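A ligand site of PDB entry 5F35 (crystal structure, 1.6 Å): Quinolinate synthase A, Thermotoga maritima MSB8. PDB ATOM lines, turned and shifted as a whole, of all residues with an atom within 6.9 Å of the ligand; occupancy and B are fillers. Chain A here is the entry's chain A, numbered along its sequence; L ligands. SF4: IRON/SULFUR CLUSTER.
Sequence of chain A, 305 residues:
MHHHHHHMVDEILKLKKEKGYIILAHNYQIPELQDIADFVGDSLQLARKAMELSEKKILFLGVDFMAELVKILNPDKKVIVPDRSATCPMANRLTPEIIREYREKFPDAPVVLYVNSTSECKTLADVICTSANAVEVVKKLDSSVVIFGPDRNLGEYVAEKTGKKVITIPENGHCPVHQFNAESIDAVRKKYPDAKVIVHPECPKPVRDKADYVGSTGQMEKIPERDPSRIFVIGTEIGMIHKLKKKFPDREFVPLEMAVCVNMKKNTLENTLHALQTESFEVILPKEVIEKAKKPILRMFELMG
SG of Cys 175 binds FE1 of the ligand (2.3 Å).
SG of Cys 88 is bound to FE4 of the ligand.
FE2 of the ligand is bound by SG of Cys 261, at 2.4 Å.
ND2 of Asn 116 lies close to S2 of the ligand (3.2 Å).
SG of Cys 175 lies close to N of Val 177 (3.4 Å).
SD of Met 90 is in hydrogen-bond range of N of Cys 175 (3.5 Å).
SG of Cys 175 lies close to ND1 of His 178, at 3.3 Å.
SG of Cys 88 sits close to N of Ala 91, at 3.7 Å.
The backbone NH (N) of Cys 261 lies within hydrogen-bond range of the side-chain carboxylate (OE2) of Glu 237 (2.8 Å).
The side-chain carboxylate (OE1) of Glu 202 lies within hydrogen-bond range of a ring nitrogen (ND1) of His 178 (3.2 Å).
A ring nitrogen (ND1) of His 26 sits at hydrogen-bond distance from the backbone NH (N) of Tyr 28.
OG1 of Thr 236 is in hydrogen-bond range of OH of Tyr 28.
The side-chain carboxylate (OE1) of Glu 202 sits close to a sulfur (S2) of the ligand.
Tyr 28 touches the ligand.
Pro 89 touches the ligand (CD to S3, 3.9 Å).
CE of Met 90 touches S2 of the ligand, at 3.997 Å.
Val 177 touches the ligand.
Hydrophobic or aromatic side chains within 4 Å of the ligand: Tyr 28, Pro 89, Met 90 and Val 177.
Within 4 Å of the ligand: Tyr 28, Cys 88, Pro 89, Met 90, Asn 116, Cys 175, Val 177, Glu 202 and Cys 261.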
ATOM      1  N   HIS A  26      22.814 -10.417 -21.398  1.00  0.00           N
ATOM      2  CA  HIS A  26      22.035  -9.726 -20.367  1.00  0.00           C
ATOM      3  C   HIS A  26      22.867  -9.441 -19.092  1.00  0.00           C
ATOM      4  O   HIS A  26      23.783 -10.196 -18.703  1.00  0.00           O
ATOM      5  CB  HIS A  26      20.754 -10.537 -19.991  1.00  0.00           C
ATOM      6  CG  HIS A  26      19.826  -9.736 -19.128  1.00  0.00           C
ATOM      7  ND1 HIS A  26      19.875  -9.828 -17.766  1.00  0.00           N
ATOM      8  CD2 HIS A  26      18.922  -8.766 -19.416  1.00  0.00           C
ATOM      9  CE1 HIS A  26      19.028  -8.961 -17.234  1.00  0.00           C
ATOM     10  NE2 HIS A  26      18.434  -8.312 -18.217  1.00  0.00           N
ATOM     11  N   TYR A  28      22.318  -9.989 -16.021  1.00  0.00           N
ATOM     12  CA  TYR A  28      22.270 -11.012 -14.963  1.00  0.00           C
ATOM     13  C   TYR A  28      23.205 -12.211 -15.300  1.00  0.00           C
ATOM     14  O   TYR A  28      23.294 -13.163 -14.548  1.00  0.00           O
ATOM     15  CB  TYR A  28      20.852 -11.527 -14.696  1.00  0.00           C
ATOM     16  CG  TYR A  28      19.878 -10.504 -14.212  1.00  0.00           C
ATOM     17  CD1 TYR A  28      20.305  -9.292 -13.631  1.00  0.00           C
ATOM     18  CD2 TYR A  28      18.497 -10.731 -14.305  1.00  0.00           C
ATOM     19  CE1 TYR A  28      19.363  -8.338 -13.174  1.00  0.00           C
ATOM     20  CE2 TYR A  28      17.574  -9.773 -13.852  1.00  0.00           C
ATOM     21  CZ  TYR A  28      18.015  -8.601 -13.298  1.00  0.00           C
ATOM     22  OH  TYR A  28      17.096  -7.669 -12.855  1.00  0.00           O
ATOM     23  N   VAL A  63      17.914 -15.461 -21.356  1.00  0.00           N
ATOM     24  CA  VAL A  63      16.818 -16.457 -21.341  1.00  0.00           C
ATOM     25  C   VAL A  63      16.001 -16.449 -22.626  1.00  0.00           C
ATOM     26  O   VAL A  63      16.087 -15.517 -23.417  1.00  0.00           O
ATOM     27  CB  VAL A  63      15.935 -16.336 -20.094  1.00  0.00           C
ATOM     28  CG1 VAL A  63      16.771 -16.598 -18.842  1.00  0.00           C
ATOM     29  CG2 VAL A  63      15.210 -14.995 -20.024  1.00  0.00           C
ATOM     30  N   PHE A  65      12.962 -16.062 -23.993  1.00  0.00           N
ATOM     31  CA  PHE A  65      12.090 -15.020 -24.535  1.00  0.00           C
ATOM     32  C   PHE A  65      12.906 -13.908 -25.202  1.00  0.00           C
ATOM     33  O   PHE A  65      12.531 -13.421 -26.274  1.00  0.00           O
ATOM     34  CB  PHE A  65      11.079 -14.452 -23.496  1.00  0.00           C
ATOM     35  CG  PHE A  65      11.656 -13.521 -22.431  1.00  0.00           C
ATOM     36  CD1 PHE A  65      12.031 -12.231 -22.735  1.00  0.00           C
ATOM     37  CD2 PHE A  65      11.748 -13.934 -21.116  1.00  0.00           C
ATOM     38  CE1 PHE A  65      12.531 -11.372 -21.785  1.00  0.00           C
ATOM     39  CE2 PHE A  65      12.252 -13.076 -20.145  1.00  0.00           C
ATOM     40  CZ  PHE A  65      12.643 -11.798 -20.488  1.00  0.00           C
ATOM     41  N   MET A  66      14.049 -13.597 -24.600  1.00  0.00           N
ATOM     42  CA  MET A  66      14.949 -12.535 -25.099  1.00  0.00           C
ATOM     43  C   MET A  66      15.604 -12.983 -26.402  1.00  0.00           C
ATOM     44  O   MET A  66      15.684 -12.217 -27.372  1.00  0.00           O
ATOM     45  CB  MET A  66      16.067 -12.210 -24.096  1.00  0.00           C
ATOM     46  CG  MET A  66      15.682 -11.731 -22.697  1.00  0.00           C
ATOM     47  SD  MET A  66      17.058 -11.606 -21.496  1.00  0.00           S
ATOM     48  CE  MET A  66      16.129 -10.916 -20.145  1.00  0.00           C
ATOM     49  N   THR A  87      14.932 -20.192 -19.242  1.00  0.00           N
ATOM     50  CA  THR A  87      13.642 -19.537 -19.469  1.00  0.00           C
ATOM     51  C   THR A  87      13.220 -18.679 -18.267  1.00  0.00           C
ATOM     52  O   THR A  87      13.886 -18.701 -17.260  1.00  0.00           O
ATOM     53  CB  THR A  87      12.578 -20.611 -19.773  1.00  0.00           C
ATOM     54  OG1 THR A  87      11.391 -19.999 -20.285  1.00  0.00           O
ATOM     55  CG2 THR A  87      12.259 -21.439 -18.538  1.00  0.00           C
ATOM     56  N   CYS A  88      12.139 -17.914 -18.406  1.00  0.00           N
ATOM     57  CA  CYS A  88      11.567 -17.100 -17.282  1.00  0.00           C
ATOM     58  C   CYS A  88      10.277 -17.733 -16.798  1.00  0.00           C
ATOM     59  O   CYS A  88       9.292 -17.786 -17.538  1.00  0.00           O
ATOM     60  CB  CYS A  88      11.312 -15.687 -17.753  1.00  0.00           C
ATOM     61  SG  CYS A  88      10.614 -14.621 -16.500  1.00  0.00           S
ATOM     62  N   PRO A  89      10.283 -18.255 -15.571  1.00  0.00           N
ATOM     63  CA  PRO A  89       9.095 -18.897 -14.993  1.00  0.00           C
ATOM     64  C   PRO A  89       7.855 -18.010 -14.942  1.00  0.00           C
ATOM     65  O   PRO A  89       6.745 -18.495 -15.119  1.00  0.00           O
ATOM     66  CB  PRO A  89       9.547 -19.265 -13.585  1.00  0.00           C
ATOM     67  CG  PRO A  89      11.007 -19.543 -13.736  1.00  0.00           C
ATOM     68  CD  PRO A  89      11.494 -18.542 -14.755  1.00  0.00           C
ATOM     69  N   MET A  90       8.062 -16.714 -14.731  1.00  0.00           N
ATOM     70  CA  MET A  90       6.950 -15.763 -14.697  1.00  0.00           C
ATOM     71  C   MET A  90       6.264 -15.658 -16.057  1.00  0.00           C
ATOM     72  O   MET A  90       5.035 -15.683 -16.153  1.00  0.00           O
ATOM     73  CB  MET A  90       7.459 -14.384 -14.262  1.00  0.00           C
ATOM     74  CG  MET A  90       6.389 -13.321 -14.260  1.00  0.00           C
ATOM     75  SD  MET A  90       7.088 -11.753 -13.749  1.00  0.00           S
ATOM     76  CE  MET A  90       7.912 -11.256 -15.252  1.00  0.00           C
ATOM     77  N   ALA A  91       7.067 -15.540 -17.107  1.00  0.00           N
ATOM     78  CA  ALA A  91       6.567 -15.424 -18.465  1.00  0.00           C
ATOM     79  C   ALA A  91       5.686 -16.608 -18.813  1.00  0.00           C
ATOM     80  O   ALA A  91       4.593 -16.466 -19.334  1.00  0.00           O
ATOM     81  CB  ALA A  91       7.722 -15.326 -19.437  1.00  0.00           C
ATOM     82  N   TYR A 114       4.815  -7.354 -21.279  1.00  0.00           N
ATOM     83  CA  TYR A 114       6.213  -7.251 -20.902  1.00  0.00           C
ATOM     84  C   TYR A 114       6.990  -8.187 -21.791  1.00  0.00           C
ATOM     85  O   TYR A 114       6.484  -9.245 -22.215  1.00  0.00           O
ATOM     86  CB  TYR A 114       6.342  -7.673 -19.444  1.00  0.00           C
ATOM     87  CG  TYR A 114       7.586  -7.370 -18.693  1.00  0.00           C
ATOM     88  CD1 TYR A 114       8.462  -6.353 -19.039  1.00  0.00           C
ATOM     89  CD2 TYR A 114       7.845  -8.062 -17.544  1.00  0.00           C
ATOM     90  CE1 TYR A 114       9.591  -6.098 -18.291  1.00  0.00           C
ATOM     91  CE2 TYR A 114       8.957  -7.798 -16.765  1.00  0.00           C
ATOM     92  CZ  TYR A 114       9.810  -6.801 -17.144  1.00  0.00           C
ATOM     93  OH  TYR A 114      10.912  -6.565 -16.341  1.00  0.00           O
ATOM     94  N   ASN A 116       9.238 -10.236 -21.040  1.00  0.00           N
ATOM     95  CA  ASN A 116       9.166 -11.505 -20.364  1.00  0.00           C
ATOM     96  C   ASN A 116       7.805 -12.166 -20.651  1.00  0.00           C
ATOM     97  O   ASN A 116       6.931 -12.086 -19.804  1.00  0.00           O
ATOM     98  CB  ASN A 116       9.294 -11.251 -18.821  1.00  0.00           C
ATOM     99  CG  ASN A 116      10.516 -10.397 -18.432  1.00  0.00           C
ATOM    100  OD1 ASN A 116      10.818  -9.360 -19.046  1.00  0.00           O
ATOM    101  ND2 ASN A 116      11.188 -10.821 -17.369  1.00  0.00           N
ATOM    102  N   ASP A 151       3.683  -9.420 -15.254  1.00  0.00           N
ATOM    103  CA  ASP A 151       4.149  -9.024 -13.911  1.00  0.00           C
ATOM    104  C   ASP A 151       3.208  -8.012 -13.260  1.00  0.00           C
ATOM    105  O   ASP A 151       3.072  -6.899 -13.729  1.00  0.00           O
ATOM    106  CB  ASP A 151       5.560  -8.470 -13.997  1.00  0.00           C
ATOM    107  CG  ASP A 151       6.260  -8.423 -12.661  1.00  0.00           C
ATOM    108  OD1 ASP A 151       5.933  -7.548 -11.891  1.00  0.00           O
ATOM    109  OD2 ASP A 151       7.207  -9.210 -12.425  1.00  0.00           O
ATOM    110  N   HIS A 174       4.346 -12.750 -11.044  1.00  0.00           N
ATOM    111  CA  HIS A 174       5.432 -12.068 -10.295  1.00  0.00           C
ATOM    112  C   HIS A 174       6.742 -12.781 -10.493  1.00  0.00           C
ATOM    113  O   HIS A 174       6.763 -13.958 -10.798  1.00  0.00           O
ATOM    114  CB  HIS A 174       5.118 -12.008  -8.794  1.00  0.00           C
ATOM    115  CG  HIS A 174       5.257 -13.313  -8.087  1.00  0.00           C
ATOM    116  ND1 HIS A 174       4.287 -14.298  -8.164  1.00  0.00           N
ATOM    117  CD2 HIS A 174       6.237 -13.806  -7.303  1.00  0.00           C
ATOM    118  CE1 HIS A 174       4.668 -15.341  -7.461  1.00  0.00           C
ATOM    119  NE2 HIS A 174       5.859 -15.065  -6.925  1.00  0.00           N
ATOM    120  N   CYS A 175       7.847 -12.037 -10.310  1.00  0.00           N
ATOM    121  CA  CYS A 175       9.205 -12.561 -10.355  1.00  0.00           C
ATOM    122  C   CYS A 175       9.620 -12.992  -8.938  1.00  0.00           C
ATOM    123  O   CYS A 175       9.684 -12.145  -8.056  1.00  0.00           O
ATOM    124  CB  CYS A 175      10.183 -11.499 -10.882  1.00  0.00           C
ATOM    125  SG  CYS A 175      11.915 -12.059 -10.744  1.00  0.00           S
ATOM    126  N   PRO A 176       9.895 -14.281  -8.721  1.00  0.00           N
ATOM    127  CA  PRO A 176      10.338 -14.714  -7.382  1.00  0.00           C
ATOM    128  C   PRO A 176      11.691 -14.126  -6.942  1.00  0.00           C
ATOM    129  O   PRO A 176      11.938 -13.939  -5.752  1.00  0.00           O
ATOM    130  CB  PRO A 176      10.408 -16.239  -7.505  1.00  0.00           C
ATOM    131  CG  PRO A 176      10.598 -16.494  -8.953  1.00  0.00           C
ATOM    132  CD  PRO A 176       9.979 -15.367  -9.717  1.00  0.00           C
ATOM    133  N   VAL A 177      12.560 -13.805  -7.901  1.00  0.00           N
ATOM    134  CA  VAL A 177      13.879 -13.277  -7.606  1.00  0.00           C
ATOM    135  C   VAL A 177      13.806 -11.893  -6.929  1.00  0.00           C
ATOM    136  O   VAL A 177      14.635 -11.561  -6.080  1.00  0.00           O
ATOM    137  CB  VAL A 177      14.750 -13.241  -8.900  1.00  0.00           C
ATOM    138  CG1 VAL A 177      16.119 -12.669  -8.618  1.00  0.00           C
ATOM    139  CG2 VAL A 177      14.868 -14.643  -9.518  1.00  0.00           C
ATOM    140  N   HIS A 178      12.791 -11.108  -7.257  1.00  0.00           N
ATOM    141  CA  HIS A 178      12.681  -9.741  -6.810  1.00  0.00           C
ATOM    142  C   HIS A 178      11.785  -9.593  -5.596  1.00  0.00           C
ATOM    143  O   HIS A 178      11.467  -8.479  -5.228  1.00  0.00           O
ATOM    144  CB  HIS A 178      12.224  -8.816  -7.959  1.00  0.00           C
ATOM    145  CG  HIS A 178      13.322  -8.514  -8.938  1.00  0.00           C
ATOM    146  ND1 HIS A 178      13.518  -9.225 -10.110  1.00  0.00           N
ATOM    147  CD2 HIS A 178      14.305  -7.574  -8.897  1.00  0.00           C
ATOM    148  CE1 HIS A 178      14.549  -8.725 -10.755  1.00  0.00           C
ATOM    149  NE2 HIS A 178      15.060  -7.734 -10.040  1.00  0.00           N
ATOM    150  N   GLU A 202       9.948  -4.599 -10.553  1.00  0.00           N
ATOM    151  CA  GLU A 202       9.389  -5.945 -10.307  1.00  0.00           C
ATOM    152  C   GLU A 202       9.342  -6.242  -8.802  1.00  0.00           C
ATOM    153  O   GLU A 202       8.755  -7.253  -8.407  1.00  0.00           O
ATOM    154  CB  GLU A 202      10.182  -7.056 -11.033  1.00  0.00           C
ATOM    155  CG  GLU A 202      10.045  -7.108 -12.545  1.00  0.00           C
ATOM    156  CD  GLU A 202      10.958  -8.164 -13.173  1.00  0.00           C
ATOM    157  OE1 GLU A 202      11.451  -9.068 -12.486  1.00  0.00           O
ATOM    158  OE2 GLU A 202      11.204  -8.101 -14.383  1.00  0.00           O
ATOM    159  N   THR A 236      18.200  -5.929  -6.907  1.00  0.00           N
ATOM    160  CA  THR A 236      17.929  -6.754  -8.099  1.00  0.00           C
ATOM    161  C   THR A 236      18.780  -8.005  -8.045  1.00  0.00           C
ATOM    162  O   THR A 236      19.458  -8.255  -7.026  1.00  0.00           O
ATOM    163  CB  THR A 236      18.113  -5.943  -9.415  1.00  0.00           C
ATOM    164  OG1 THR A 236      17.411  -6.577 -10.513  1.00  0.00           O
ATOM    165  CG2 THR A 236      19.566  -5.682  -9.749  1.00  0.00           C
ATOM    166  N   GLU A 237      18.744  -8.775  -9.138  1.00  0.00           N
ATOM    167  CA  GLU A 237      19.528 -10.012  -9.271  1.00  0.00           C
ATOM    168  C   GLU A 237      21.011  -9.710  -9.153  1.00  0.00           C
ATOM    169  O   GLU A 237      21.554  -8.699  -9.732  1.00  0.00           O
ATOM    170  CB  GLU A 237      19.163 -10.746 -10.583  1.00  0.00           C
ATOM    171  CG  GLU A 237      19.359 -12.247 -10.605  1.00  0.00           C
ATOM    172  CD  GLU A 237      20.741 -12.718 -10.972  1.00  0.00           C
ATOM    173  OE1 GLU A 237      21.585 -11.878 -11.423  1.00  0.00           O
ATOM    174  OE2 GLU A 237      20.973 -13.951 -10.809  1.00  0.00           O
ATOM    175  N   VAL A 260      19.230 -14.714  -6.722  1.00  0.00           N
ATOM    176  CA  VAL A 260      19.819 -15.403  -7.881  1.00  0.00           C
ATOM    177  C   VAL A 260      18.717 -15.910  -8.794  1.00  0.00           C
ATOM    178  O   VAL A 260      17.777 -16.555  -8.344  1.00  0.00           O
ATOM    179  CB  VAL A 260      20.720 -16.572  -7.450  1.00  0.00           C
ATOM    180  CG1 VAL A 260      21.415 -17.199  -8.645  1.00  0.00           C
ATOM    181  CG2 VAL A 260      21.744 -16.089  -6.432  1.00  0.00           C
ATOM    182  N   CYS A 261      18.858 -15.650 -10.104  1.00  0.00           N
ATOM    183  CA  CYS A 261      17.932 -16.191 -11.116  1.00  0.00           C
ATOM    184  C   CYS A 261      18.593 -17.465 -11.627  1.00  0.00           C
ATOM    185  O   CYS A 261      19.569 -17.379 -12.337  1.00  0.00           O
ATOM    186  CB  CYS A 261      17.704 -15.226 -12.279  1.00  0.00           C
ATOM    187  SG  CYS A 261      16.572 -15.953 -13.509  1.00  0.00           S
ATOM    188  N   VAL A 262      18.083 -18.630 -11.225  1.00  0.00           N
ATOM    189  CA  VAL A 262      18.720 -19.899 -11.572  1.00  0.00           C
ATOM    190  C   VAL A 262      18.789 -20.082 -13.087  1.00  0.00           C
ATOM    191  O   VAL A 262      19.776 -20.590 -13.612  1.00  0.00           O
ATOM    192  CB  VAL A 262      18.086 -21.095 -10.806  1.00  0.00           C
ATOM    193  CG1 VAL A 262      18.685 -22.419 -11.203  1.00  0.00           C
ATOM    194  CG2 VAL A 262      18.300 -20.896  -9.322  1.00  0.00           C
ATOM    195  N   ASN A 263      17.754 -19.652 -13.794  1.00  0.00           N
ATOM    196  CA  ASN A 263      17.776 -19.730 -15.263  1.00  0.00           C
ATOM    197  C   ASN A 263      18.852 -18.880 -15.913  1.00  0.00           C
ATOM    198  O   ASN A 263      19.514 -19.342 -16.849  1.00  0.00           O
ATOM    199  CB  ASN A 263      16.416 -19.423 -15.845  1.00  0.00           C
ATOM    200  CG  ASN A 263      15.503 -20.608 -15.795  1.00  0.00           C
ATOM    201  OD1 ASN A 263      15.537 -21.472 -16.678  1.00  0.00           O
ATOM    202  ND2 ASN A 263      14.645 -20.639 -14.769  1.00  0.00           N
ATOM    203  N   MET A 264      19.081 -17.680 -15.409  1.00  0.00           N
ATOM    204  CA  MET A 264      20.168 -16.817 -15.923  1.00  0.00           C
ATOM    205  C   MET A 264      21.533 -17.487 -15.707  1.00  0.00           C
ATOM    206  O   MET A 264      22.422 -17.346 -16.544  1.00  0.00           O
ATOM    207  CB  MET A 264      20.133 -15.432 -15.325  1.00  0.00           C
ATOM    208  CG  MET A 264      19.010 -14.567 -15.922  1.00  0.00           C
ATOM    209  SD  MET A 264      19.415 -13.936 -17.559  1.00  0.00           S
ATOM    210  CE  MET A 264      18.026 -12.844 -17.905  1.00  0.00           C
HETATM  211 FE1  SF4 L   1      12.804 -12.878 -12.648  1.00  0.00          FE
HETATM  212 FE2  SF4 L   1      14.786 -14.469 -13.896  1.00  0.00          FE
HETATM  213 FE3  SF4 L   1      14.084 -11.898 -14.830  1.00  0.00          FE
HETATM  214 FE4  SF4 L   1      12.327 -13.945 -15.109  1.00  0.00          FE
HETATM  215  S1  SF4 L   1      14.429 -13.821 -16.104  1.00  0.00           S
HETATM  216  S2  SF4 L   1      11.784 -11.798 -14.422  1.00  0.00           S
HETATM  217  S3  SF4 L   1      12.696 -15.196 -13.118  1.00  0.00           S
HETATM  218  S4  SF4 L   1      15.112 -12.429 -12.741  1.00  0.00           S
